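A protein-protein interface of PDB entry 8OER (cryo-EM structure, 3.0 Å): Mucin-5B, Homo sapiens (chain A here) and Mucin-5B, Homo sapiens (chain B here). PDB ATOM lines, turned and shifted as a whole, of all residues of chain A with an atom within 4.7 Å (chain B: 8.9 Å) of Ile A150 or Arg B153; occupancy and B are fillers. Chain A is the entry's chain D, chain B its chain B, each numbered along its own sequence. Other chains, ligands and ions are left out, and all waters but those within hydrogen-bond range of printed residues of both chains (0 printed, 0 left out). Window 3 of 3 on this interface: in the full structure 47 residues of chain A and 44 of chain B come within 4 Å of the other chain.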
ATOM      1  N   GLU A 126     -31.201  13.842  24.078  1.00  0.00           N
ATOM      2  CA  GLU A 126     -31.103  12.690  24.959  1.00  0.00           C
ATOM      3  C   GLU A 126     -32.486  12.138  25.264  1.00  0.00           C
ATOM      4  O   GLU A 126     -33.358  12.862  25.752  1.00  0.00           O
ATOM      5  CB  GLU A 126     -30.395  13.081  26.250  1.00  0.00           C
ATOM      6  CG  GLU A 126     -28.902  12.976  26.172  1.00  0.00           C
ATOM      7  CD  GLU A 126     -28.432  11.593  26.504  1.00  0.00           C
ATOM      8  OE1 GLU A 126     -28.949  10.636  25.901  1.00  0.00           O
ATOM      9  OE2 GLU A 126     -27.549  11.460  27.367  1.00  0.00           O
ATOM     10  N   GLU A 148     -28.569   8.802  22.846  1.00  0.00           N
ATOM     11  CA  GLU A 148     -28.624   9.901  21.895  1.00  0.00           C
ATOM     12  C   GLU A 148     -27.619   9.622  20.791  1.00  0.00           C
ATOM     13  O   GLU A 148     -26.614   8.942  20.999  1.00  0.00           O
ATOM     14  CB  GLU A 148     -28.333  11.241  22.556  1.00  0.00           C
ATOM     15  CG  GLU A 148     -27.118  11.210  23.420  1.00  0.00           C
ATOM     16  CD  GLU A 148     -25.976  11.960  22.806  1.00  0.00           C
ATOM     17  OE1 GLU A 148     -26.157  12.516  21.706  1.00  0.00           O
ATOM     18  OE2 GLU A 148     -24.899  11.994  23.421  1.00  0.00           O
ATOM     19  N   ASN A 149     -27.892  10.169  19.615  1.00  0.00           N
ATOM     20  CA  ASN A 149     -27.188   9.778  18.401  1.00  0.00           C
ATOM     21  C   ASN A 149     -25.943  10.635  18.213  1.00  0.00           C
ATOM     22  O   ASN A 149     -26.037  11.838  17.956  1.00  0.00           O
ATOM     23  CB  ASN A 149     -28.120   9.893  17.204  1.00  0.00           C
ATOM     24  CG  ASN A 149     -29.151   8.799  17.177  1.00  0.00           C
ATOM     25  OD1 ASN A 149     -28.980   7.758  17.806  1.00  0.00           O
ATOM     26  ND2 ASN A 149     -30.233   9.025  16.450  1.00  0.00           N
ATOM     27  N   ILE A 150     -24.778  10.008  18.322  1.00  0.00           N
ATOM     28  CA  ILE A 150     -23.502  10.674  18.084  1.00  0.00           C
ATOM     29  C   ILE A 150     -23.200  10.685  16.594  1.00  0.00           C
ATOM     30  O   ILE A 150     -23.391   9.669  15.915  1.00  0.00           O
ATOM     31  CB  ILE A 150     -22.356   9.982  18.834  1.00  0.00           C
ATOM     32  CG1 ILE A 150     -22.764   9.692  20.268  1.00  0.00           C
ATOM     33  CG2 ILE A 150     -21.108  10.837  18.785  1.00  0.00           C
ATOM     34  CD1 ILE A 150     -23.095  10.915  21.029  1.00  0.00           C
ATOM     35  N   PRO A 151     -22.771  11.796  16.043  1.00  0.00           N
ATOM     36  CA  PRO A 151     -22.072  11.748  14.758  1.00  0.00           C
ATOM     37  C   PRO A 151     -20.583  11.576  14.998  1.00  0.00           C
ATOM     38  O   PRO A 151     -19.999  12.323  15.787  1.00  0.00           O
ATOM     39  CB  PRO A 151     -22.412  13.099  14.127  1.00  0.00           C
ATOM     40  CG  PRO A 151     -22.608  13.994  15.296  1.00  0.00           C
ATOM     41  CD  PRO A 151     -23.172  13.161  16.409  1.00  0.00           C
ATOM     42  N   CYS A 152     -19.957  10.597  14.349  1.00  0.00           N
ATOM     43  CA  CYS A 152     -18.615  10.185  14.739  1.00  0.00           C
ATOM     44  C   CYS A 152     -17.500  10.985  14.078  1.00  0.00           C
ATOM     45  O   CYS A 152     -16.345  10.858  14.495  1.00  0.00           O
ATOM     46  CB  CYS A 152     -18.414   8.695  14.445  1.00  0.00           C
ATOM     47  SG  CYS A 152     -18.447   8.247  12.704  1.00  0.00           S
ATOM     48  N   THR A 158     -26.342  10.321  11.837  1.00  0.00           N
ATOM     49  CA  THR A 158     -25.833   9.589  12.988  1.00  0.00           C
ATOM     50  C   THR A 158     -24.814   8.552  12.543  1.00  0.00           C
ATOM     51  O   THR A 158     -24.939   7.958  11.470  1.00  0.00           O
ATOM     52  CB  THR A 158     -26.978   8.902  13.718  1.00  0.00           C
ATOM     53  OG1 THR A 158     -27.379   7.749  12.976  1.00  0.00           O
ATOM     54  CG2 THR A 158     -28.161   9.835  13.773  1.00  0.00           C
ATOM     55  N   CYS A 159     -23.796   8.335  13.372  1.00  0.00           N
ATOM     56  CA  CYS A 159     -22.774   7.346  13.090  1.00  0.00           C
ATOM     57  C   CYS A 159     -22.573   6.368  14.229  1.00  0.00           C
ATOM     58  O   CYS A 159     -22.211   5.216  13.977  1.00  0.00           O
ATOM     59  CB  CYS A 159     -21.441   8.039  12.774  1.00  0.00           C
ATOM     60  SG  CYS A 159     -20.013   6.961  12.591  1.00  0.00           S
ATOM     61  N   SER A 160     -22.812   6.787  15.463  1.00  0.00           N
ATOM     62  CA  SER A 160     -22.788   5.898  16.612  1.00  0.00           C
ATOM     63  C   SER A 160     -23.760   6.452  17.643  1.00  0.00           C
ATOM     64  O   SER A 160     -24.446   7.447  17.404  1.00  0.00           O
ATOM     65  CB  SER A 160     -21.376   5.756  17.182  1.00  0.00           C
ATOM     66  OG  SER A 160     -21.251   4.557  17.922  1.00  0.00           O
ATOM     67  N   LYS A 161     -23.820   5.800  18.795  1.00  0.00           N
ATOM     68  CA  LYS A 161     -24.737   6.193  19.849  1.00  0.00           C
ATOM     69  C   LYS A 161     -23.962   6.525  21.113  1.00  0.00           C
ATOM     70  O   LYS A 161     -22.731   6.527  21.135  1.00  0.00           O
ATOM     71  CB  LYS A 161     -25.761   5.089  20.125  1.00  0.00           C
ATOM     72  CG  LYS A 161     -27.012   5.199  19.276  1.00  0.00           C
ATOM     73  CD  LYS A 161     -28.126   4.332  19.825  1.00  0.00           C
ATOM     74  CE  LYS A 161     -29.273   4.238  18.841  1.00  0.00           C
ATOM     75  NZ  LYS A 161     -29.804   5.582  18.504  1.00  0.00           N
ATOM     76  N   ALA A 162     -24.706   6.836  22.168  1.00  0.00           N
ATOM     77  CA  ALA A 162     -24.139   7.087  23.484  1.00  0.00           C
ATOM     78  C   ALA A 162     -25.178   6.708  24.519  1.00  0.00           C
ATOM     79  O   ALA A 162     -26.290   7.236  24.506  1.00  0.00           O
ATOM     80  CB  ALA A 162     -23.730   8.546  23.652  1.00  0.00           C
ATOM     81  N   LYS A 164     -26.361   6.009  28.601  1.00  0.00           N
ATOM     82  CA  LYS A 164     -26.135   6.387  29.992  1.00  0.00           C
ATOM     83  C   LYS A 164     -26.910   5.417  30.872  1.00  0.00           C
ATOM     84  O   LYS A 164     -28.046   5.689  31.256  1.00  0.00           O
ATOM     85  CB  LYS A 164     -26.542   7.815  30.237  1.00  0.00           C
ATOM     86  CG  LYS A 164     -25.631   8.823  29.582  1.00  0.00           C
ATOM     87  CD  LYS A 164     -26.123  10.228  29.847  1.00  0.00           C
ATOM     88  CE  LYS A 164     -25.140  11.266  29.362  1.00  0.00           C
ATOM     89  NZ  LYS A 164     -25.750  12.622  29.380  1.00  0.00           N
ATOM     90  N   ALA B 111     -15.569  23.061  14.037  1.00  0.00           N
ATOM     91  CA  ALA B 111     -15.514  21.725  14.615  1.00  0.00           C
ATOM     92  C   ALA B 111     -16.145  20.734  13.658  1.00  0.00           C
ATOM     93  O   ALA B 111     -17.340  20.825  13.370  1.00  0.00           O
ATOM     94  CB  ALA B 111     -16.219  21.683  15.968  1.00  0.00           C
ATOM     95  N   GLN B 112     -15.334  19.800  13.170  1.00  0.00           N
ATOM     96  CA  GLN B 112     -15.828  18.619  12.474  1.00  0.00           C
ATOM     97  C   GLN B 112     -16.679  19.007  11.271  1.00  0.00           C
ATOM     98  O   GLN B 112     -17.717  18.405  10.997  1.00  0.00           O
ATOM     99  CB  GLN B 112     -16.614  17.731  13.440  1.00  0.00           C
ATOM    100  CG  GLN B 112     -15.791  17.100  14.574  1.00  0.00           C
ATOM    101  CD  GLN B 112     -14.709  16.134  14.122  1.00  0.00           C
ATOM    102  OE1 GLN B 112     -14.071  16.314  13.088  1.00  0.00           O
ATOM    103  NE2 GLN B 112     -14.481  15.105  14.925  1.00  0.00           N
ATOM    104  N   ARG B 136     -28.958  19.686  16.383  1.00  0.00           N
ATOM    105  CA  ARG B 136     -28.633  18.691  15.374  1.00  0.00           C
ATOM    106  C   ARG B 136     -27.864  17.575  16.066  1.00  0.00           C
ATOM    107  O   ARG B 136     -27.391  17.739  17.190  1.00  0.00           O
ATOM    108  CB  ARG B 136     -27.821  19.309  14.234  1.00  0.00           C
ATOM    109  CG  ARG B 136     -27.963  18.608  12.907  1.00  0.00           C
ATOM    110  CD  ARG B 136     -29.408  18.482  12.500  1.00  0.00           C
ATOM    111  NE  ARG B 136     -30.142  19.723  12.700  1.00  0.00           N
ATOM    112  CZ  ARG B 136     -30.105  20.753  11.867  1.00  0.00           C
ATOM    113  NH1 ARG B 136     -29.352  20.735  10.780  1.00  0.00           N
ATOM    114  NH2 ARG B 136     -30.847  21.823  12.128  1.00  0.00           N
ATOM    115  N   THR B 137     -27.723  16.449  15.379  1.00  0.00           N
ATOM    116  CA  THR B 137     -27.020  15.317  15.963  1.00  0.00           C
ATOM    117  C   THR B 137     -25.664  15.746  16.495  1.00  0.00           C
ATOM    118  O   THR B 137     -24.815  16.226  15.741  1.00  0.00           O
ATOM    119  CB  THR B 137     -26.856  14.216  14.924  1.00  0.00           C
ATOM    120  OG1 THR B 137     -26.055  14.709  13.848  1.00  0.00           O
ATOM    121  CG2 THR B 137     -28.210  13.803  14.384  1.00  0.00           C
ATOM    122  N   GLY B 138     -25.484  15.607  17.808  1.00  0.00           N
ATOM    123  CA  GLY B 138     -24.246  15.956  18.472  1.00  0.00           C
ATOM    124  C   GLY B 138     -24.101  17.405  18.884  1.00  0.00           C
ATOM    125  O   GLY B 138     -23.402  17.683  19.865  1.00  0.00           O
ATOM    126  N   LEU B 139     -24.741  18.338  18.186  1.00  0.00           N
ATOM    127  CA  LEU B 139     -24.582  19.760  18.450  1.00  0.00           C
ATOM    128  C   LEU B 139     -25.891  20.372  18.918  1.00  0.00           C
ATOM    129  O   LEU B 139     -26.951  20.082  18.367  1.00  0.00           O
ATOM    130  CB  LEU B 139     -24.083  20.493  17.205  1.00  0.00           C
ATOM    131  CG  LEU B 139     -24.222  22.011  17.211  1.00  0.00           C
ATOM    132  CD1 LEU B 139     -23.009  22.643  16.606  1.00  0.00           C
ATOM    133  CD2 LEU B 139     -25.439  22.426  16.415  1.00  0.00           C
ATOM    134  N   LEU B 140     -25.821  21.228  19.932  1.00  0.00           N
ATOM    135  CA  LEU B 140     -26.991  22.012  20.299  1.00  0.00           C
ATOM    136  C   LEU B 140     -26.543  23.366  20.821  1.00  0.00           C
ATOM    137  O   LEU B 140     -25.649  23.448  21.668  1.00  0.00           O
ATOM    138  CB  LEU B 140     -27.866  21.285  21.326  1.00  0.00           C
ATOM    139  CG  LEU B 140     -27.472  21.179  22.793  1.00  0.00           C
ATOM    140  CD1 LEU B 140     -28.652  20.673  23.589  1.00  0.00           C
ATOM    141  CD2 LEU B 140     -26.303  20.233  22.949  1.00  0.00           C
ATOM    142  N   VAL B 150     -23.054  26.622  23.439  1.00  0.00           N
ATOM    143  CA  VAL B 150     -22.857  25.728  22.309  1.00  0.00           C
ATOM    144  C   VAL B 150     -22.229  24.453  22.847  1.00  0.00           C
ATOM    145  O   VAL B 150     -21.064  24.454  23.260  1.00  0.00           O
ATOM    146  CB  VAL B 150     -21.959  26.360  21.243  1.00  0.00           C
ATOM    147  CG1 VAL B 150     -21.664  25.353  20.160  1.00  0.00           C
ATOM    148  CG2 VAL B 150     -22.590  27.624  20.690  1.00  0.00           C
ATOM    149  N   SER B 151     -22.979  23.360  22.845  1.00  0.00           N
ATOM    150  CA  SER B 151     -22.473  22.085  23.329  1.00  0.00           C
ATOM    151  C   SER B 151     -22.383  21.117  22.163  1.00  0.00           C
ATOM    152  O   SER B 151     -23.389  20.847  21.497  1.00  0.00           O
ATOM    153  CB  SER B 151     -23.363  21.525  24.433  1.00  0.00           C
ATOM    154  OG  SER B 151     -22.888  20.265  24.861  1.00  0.00           O
ATOM    155  N   ILE B 152     -21.180  20.613  21.913  1.00  0.00           N
ATOM    156  CA  ILE B 152     -20.916  19.624  20.876  1.00  0.00           C
ATOM    157  C   ILE B 152     -20.527  18.349  21.610  1.00  0.00           C
ATOM    158  O   ILE B 152     -19.431  18.247  22.163  1.00  0.00           O
ATOM    159  CB  ILE B 152     -19.816  20.084  19.919  1.00  0.00           C
ATOM    160  CG1 ILE B 152     -20.128  21.470  19.370  1.00  0.00           C
ATOM    161  CG2 ILE B 152     -19.660  19.109  18.775  1.00  0.00           C
ATOM    162  CD1 ILE B 152     -18.969  22.090  18.632  1.00  0.00           C
ATOM    163  N   ARG B 153     -21.432  17.381  21.617  1.00  0.00           N
ATOM    164  CA  ARG B 153     -21.315  16.249  22.521  1.00  0.00           C
ATOM    165  C   ARG B 153     -20.054  15.447  22.209  1.00  0.00           C
ATOM    166  O   ARG B 153     -19.687  15.279  21.048  1.00  0.00           O
ATOM    167  CB  ARG B 153     -22.589  15.413  22.408  1.00  0.00           C
ATOM    168  CG  ARG B 153     -22.440  13.933  22.373  1.00  0.00           C
ATOM    169  CD  ARG B 153     -22.168  13.361  23.745  1.00  0.00           C
ATOM    170  NE  ARG B 153     -23.348  13.221  24.585  1.00  0.00           N
ATOM    171  CZ  ARG B 153     -23.342  12.631  25.771  1.00  0.00           C
ATOM    172  NH1 ARG B 153     -22.242  12.093  26.269  1.00  0.00           N
ATOM    173  NH2 ARG B 153     -24.474  12.557  26.462  1.00  0.00           N
ATOM    174  N   LEU B 154     -19.368  14.986  23.258  1.00  0.00           N
ATOM    175  CA  LEU B 154     -18.003  14.449  23.242  1.00  0.00           C
ATOM    176  C   LEU B 154     -16.941  15.421  22.738  1.00  0.00           C
ATOM    177  O   LEU B 154     -15.782  15.008  22.596  1.00  0.00           O
ATOM    178  CB  LEU B 154     -17.822  13.142  22.444  1.00  0.00           C
ATOM    179  CG  LEU B 154     -18.175  11.701  22.842  1.00  0.00           C
ATOM    180  CD1 LEU B 154     -17.103  11.209  23.808  1.00  0.00           C
ATOM    181  CD2 LEU B 154     -19.507  11.549  23.459  1.00  0.00           C
ATOM    182  N   VAL B 155     -17.263  16.688  22.486  1.00  0.00           N
ATOM    183  CA  VAL B 155     -16.218  17.599  22.032  1.00  0.00           C
ATOM    184  C   VAL B 155     -16.035  18.728  23.036  1.00  0.00           C
ATOM    185  O   VAL B 155     -14.990  18.828  23.688  1.00  0.00           O
ATOM    186  CB  VAL B 155     -16.529  18.151  20.630  1.00  0.00           C
ATOM    187  CG1 VAL B 155     -15.481  19.152  20.210  1.00  0.00           C
ATOM    188  CG2 VAL B 155     -16.592  17.026  19.634  1.00  0.00           C
ATOM    189  N   LEU B 156     -17.054  19.557  23.213  1.00  0.00           N
ATOM    190  CA  LEU B 156     -16.808  20.752  23.998  1.00  0.00           C
ATOM    191  C   LEU B 156     -18.112  21.374  24.465  1.00  0.00           C
ATOM    192  O   LEU B 156     -19.203  21.034  24.000  1.00  0.00           O
ATOM    193  CB  LEU B 156     -15.977  21.766  23.200  1.00  0.00           C
ATOM    194  CG  LEU B 156     -16.493  22.311  21.868  1.00  0.00           C
ATOM    195  CD1 LEU B 156     -17.456  23.458  22.050  1.00  0.00           C
ATOM    196  CD2 LEU B 156     -15.334  22.753  21.022  1.00  0.00           C
ATOM    197  N   THR B 157     -17.962  22.307  25.394  1.00  0.00           N
ATOM    198  CA  THR B 157     -19.057  23.094  25.936  1.00  0.00           C
ATOM    199  C   THR B 157     -18.566  24.530  25.929  1.00  0.00           C
ATOM    200  O   THR B 157     -17.488  24.811  26.450  1.00  0.00           O
ATOM    201  CB  THR B 157     -19.417  22.635  27.348  1.00  0.00           C
ATOM    202  OG1 THR B 157     -19.532  21.209  27.371  1.00  0.00           O
ATOM    203  CG2 THR B 157     -20.725  23.238  27.796  1.00  0.00           C
ATOM    204  N   ASP B 171     -13.375  17.805  26.632  1.00  0.00           N
ATOM    205  CA  ASP B 171     -13.335  16.414  27.030  1.00  0.00           C
ATOM    206  C   ASP B 171     -11.960  16.083  27.597  1.00  0.00           C
ATOM    207  O   ASP B 171     -10.972  16.739  27.267  1.00  0.00           O
ATOM    208  CB  ASP B 171     -13.631  15.509  25.842  1.00  0.00           C
ATOM    209  CG  ASP B 171     -13.975  14.097  26.257  1.00  0.00           C
ATOM    210  OD1 ASP B 171     -15.114  13.869  26.709  1.00  0.00           O
ATOM    211  OD2 ASP B 171     -13.098  13.217  26.155  1.00  0.00           O
ATOM    212  N   LYS B 173     -10.294  13.589  26.730  1.00  0.00           N
ATOM    213  CA  LYS B 173      -9.498  12.928  25.706  1.00  0.00           C
ATOM    214  C   LYS B 173      -8.592  13.883  24.944  1.00  0.00           C
ATOM    215  O   LYS B 173      -7.650  13.420  24.297  1.00  0.00           O
ATOM    216  CB  LYS B 173     -10.403  12.175  24.730  1.00  0.00           C
ATOM    217  CG  LYS B 173     -10.687  12.887  23.429  1.00  0.00           C
ATOM    218  CD  LYS B 173     -11.391  11.949  22.462  1.00  0.00           C
ATOM    219  CE  LYS B 173     -12.893  12.155  22.460  1.00  0.00           C
ATOM    220  NZ  LYS B 173     -13.274  13.511  21.995  1.00  0.00           N
ATOM    221  N   TYR B 174      -8.834  15.191  25.012  1.00  0.00           N
ATOM    222  CA  TYR B 174      -7.962  16.163  24.374  1.00  0.00           C
ATOM    223  C   TYR B 174      -6.837  16.607  25.283  1.00  0.00           C
ATOM    224  O   TYR B 174      -6.299  17.702  25.101  1.00  0.00           O
ATOM    225  CB  TYR B 174      -8.750  17.384  23.906  1.00  0.00           C
ATOM    226  CG  TYR B 174      -9.915  17.026  23.041  1.00  0.00           C
ATOM    227  CD1 TYR B 174     -11.160  16.807  23.588  1.00  0.00           C
ATOM    228  CD2 TYR B 174      -9.758  16.843  21.687  1.00  0.00           C
ATOM    229  CE1 TYR B 174     -12.226  16.462  22.804  1.00  0.00           C
ATOM    230  CE2 TYR B 174     -10.817  16.496  20.895  1.00  0.00           C
ATOM    231  CZ  TYR B 174     -12.049  16.303  21.460  1.00  0.00           C
ATOM    232  OH  TYR B 174     -13.116  15.950  20.675  1.00  0.00           O
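NH2 of Arg B153 is in salt-bridge range of OE2 of Glu A126.
NZ of Lys A164 sits close to NH2 of Arg B153 (3.2 Å).
NH2 of Arg B153 is in salt-bridge range of OE2 of Glu A148.
The side-chain amino group (NZ) of Lys A164 is in salt-bridge range of the side-chain carboxylate (OE2) of Glu A126, 2.9 Å away.
SG of Cys A152 forms a disulfide with SG of Cys A159 (2.0 Å).
O of Ile A150 is in hydrogen-bond range of N of Cys A159 (2.9 Å).
The backbone NH (N) of Ile A150 is in hydrogen-bond range of the backbone carbonyl oxygen (O) of Ser A160.
The backbone carbonyl oxygen (O) of Gly B138 sits at hydrogen-bond distance from the backbone NH (N) of Arg B153, at 2.7 Å.
The side-chain amide oxygen (OD1) of Asn A149 is in hydrogen-bond range of the side-chain amino group (NZ) of Lys A161, 2.4 Å away.
CB of Thr B137 touches O of Asn A149 (3.9 Å).
Asn A149 touches Gly B138 (O to N, 3.8 Å).
Ile A150 touches Arg B153 (CD1 to CG, 3.4 Å).
CG of Pro A151 touches O of Thr B137 (3.2 Å).
CA of Gly B138 touches CD of Pro A151 (3.6 Å).
Of the printed residues of chain B, Glu A126 touches Arg B153 (3.4 Å).
Of the printed residues of chain B, Asn A149 touches Thr B137 (3.9 Å) and Gly B138 (3.8 Å).
Of the printed residues of chain B, Ile A150 touches Arg B153 (3.4 Å).
Pro A151 touches just these residues of chain B: Thr B137 and Gly B138.
Lys A161 touches none of the printed residues of chain B.
Ala A162 touches none of the printed residues of chain B.
Printed residues of chain A within 4 Å of Thr B137: Asn A149 and Pro A151.
Printed residues of chain A within 4 Å of Gly B138: Asn A149 (3.8 Å) and Pro A151 (3.6 Å).
Arg B153 touches just these residues of chain A: Glu A126 (3.4 Å), Glu A148 (2.3 Å), Ile A150 (3.4 Å) and Lys A164 (3.2 Å).
The nearest residue of chain B that does not touch Ile A150 is Leu B154 (4.4 Å).
The nearest residue of chain A that does not touch Arg B153 is Ala A162 (4.6 Å).
Of the 12 printed residues of chain A, 6 touch a printed residue of chain B.
Along chain B the printed residues that touch a printed residue of chain A span positions 137 to 153.
Among the printed residues, 8 pairs touch across the chains.
Among the printed residues, Asp or Glu carboxylates within 4 Å of a Lys or Arg side-chain nitrogen of the other chain: Glu A126 with Arg B153 (3.4 Å) and Glu A148 with Arg B153 (2.3 Å).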
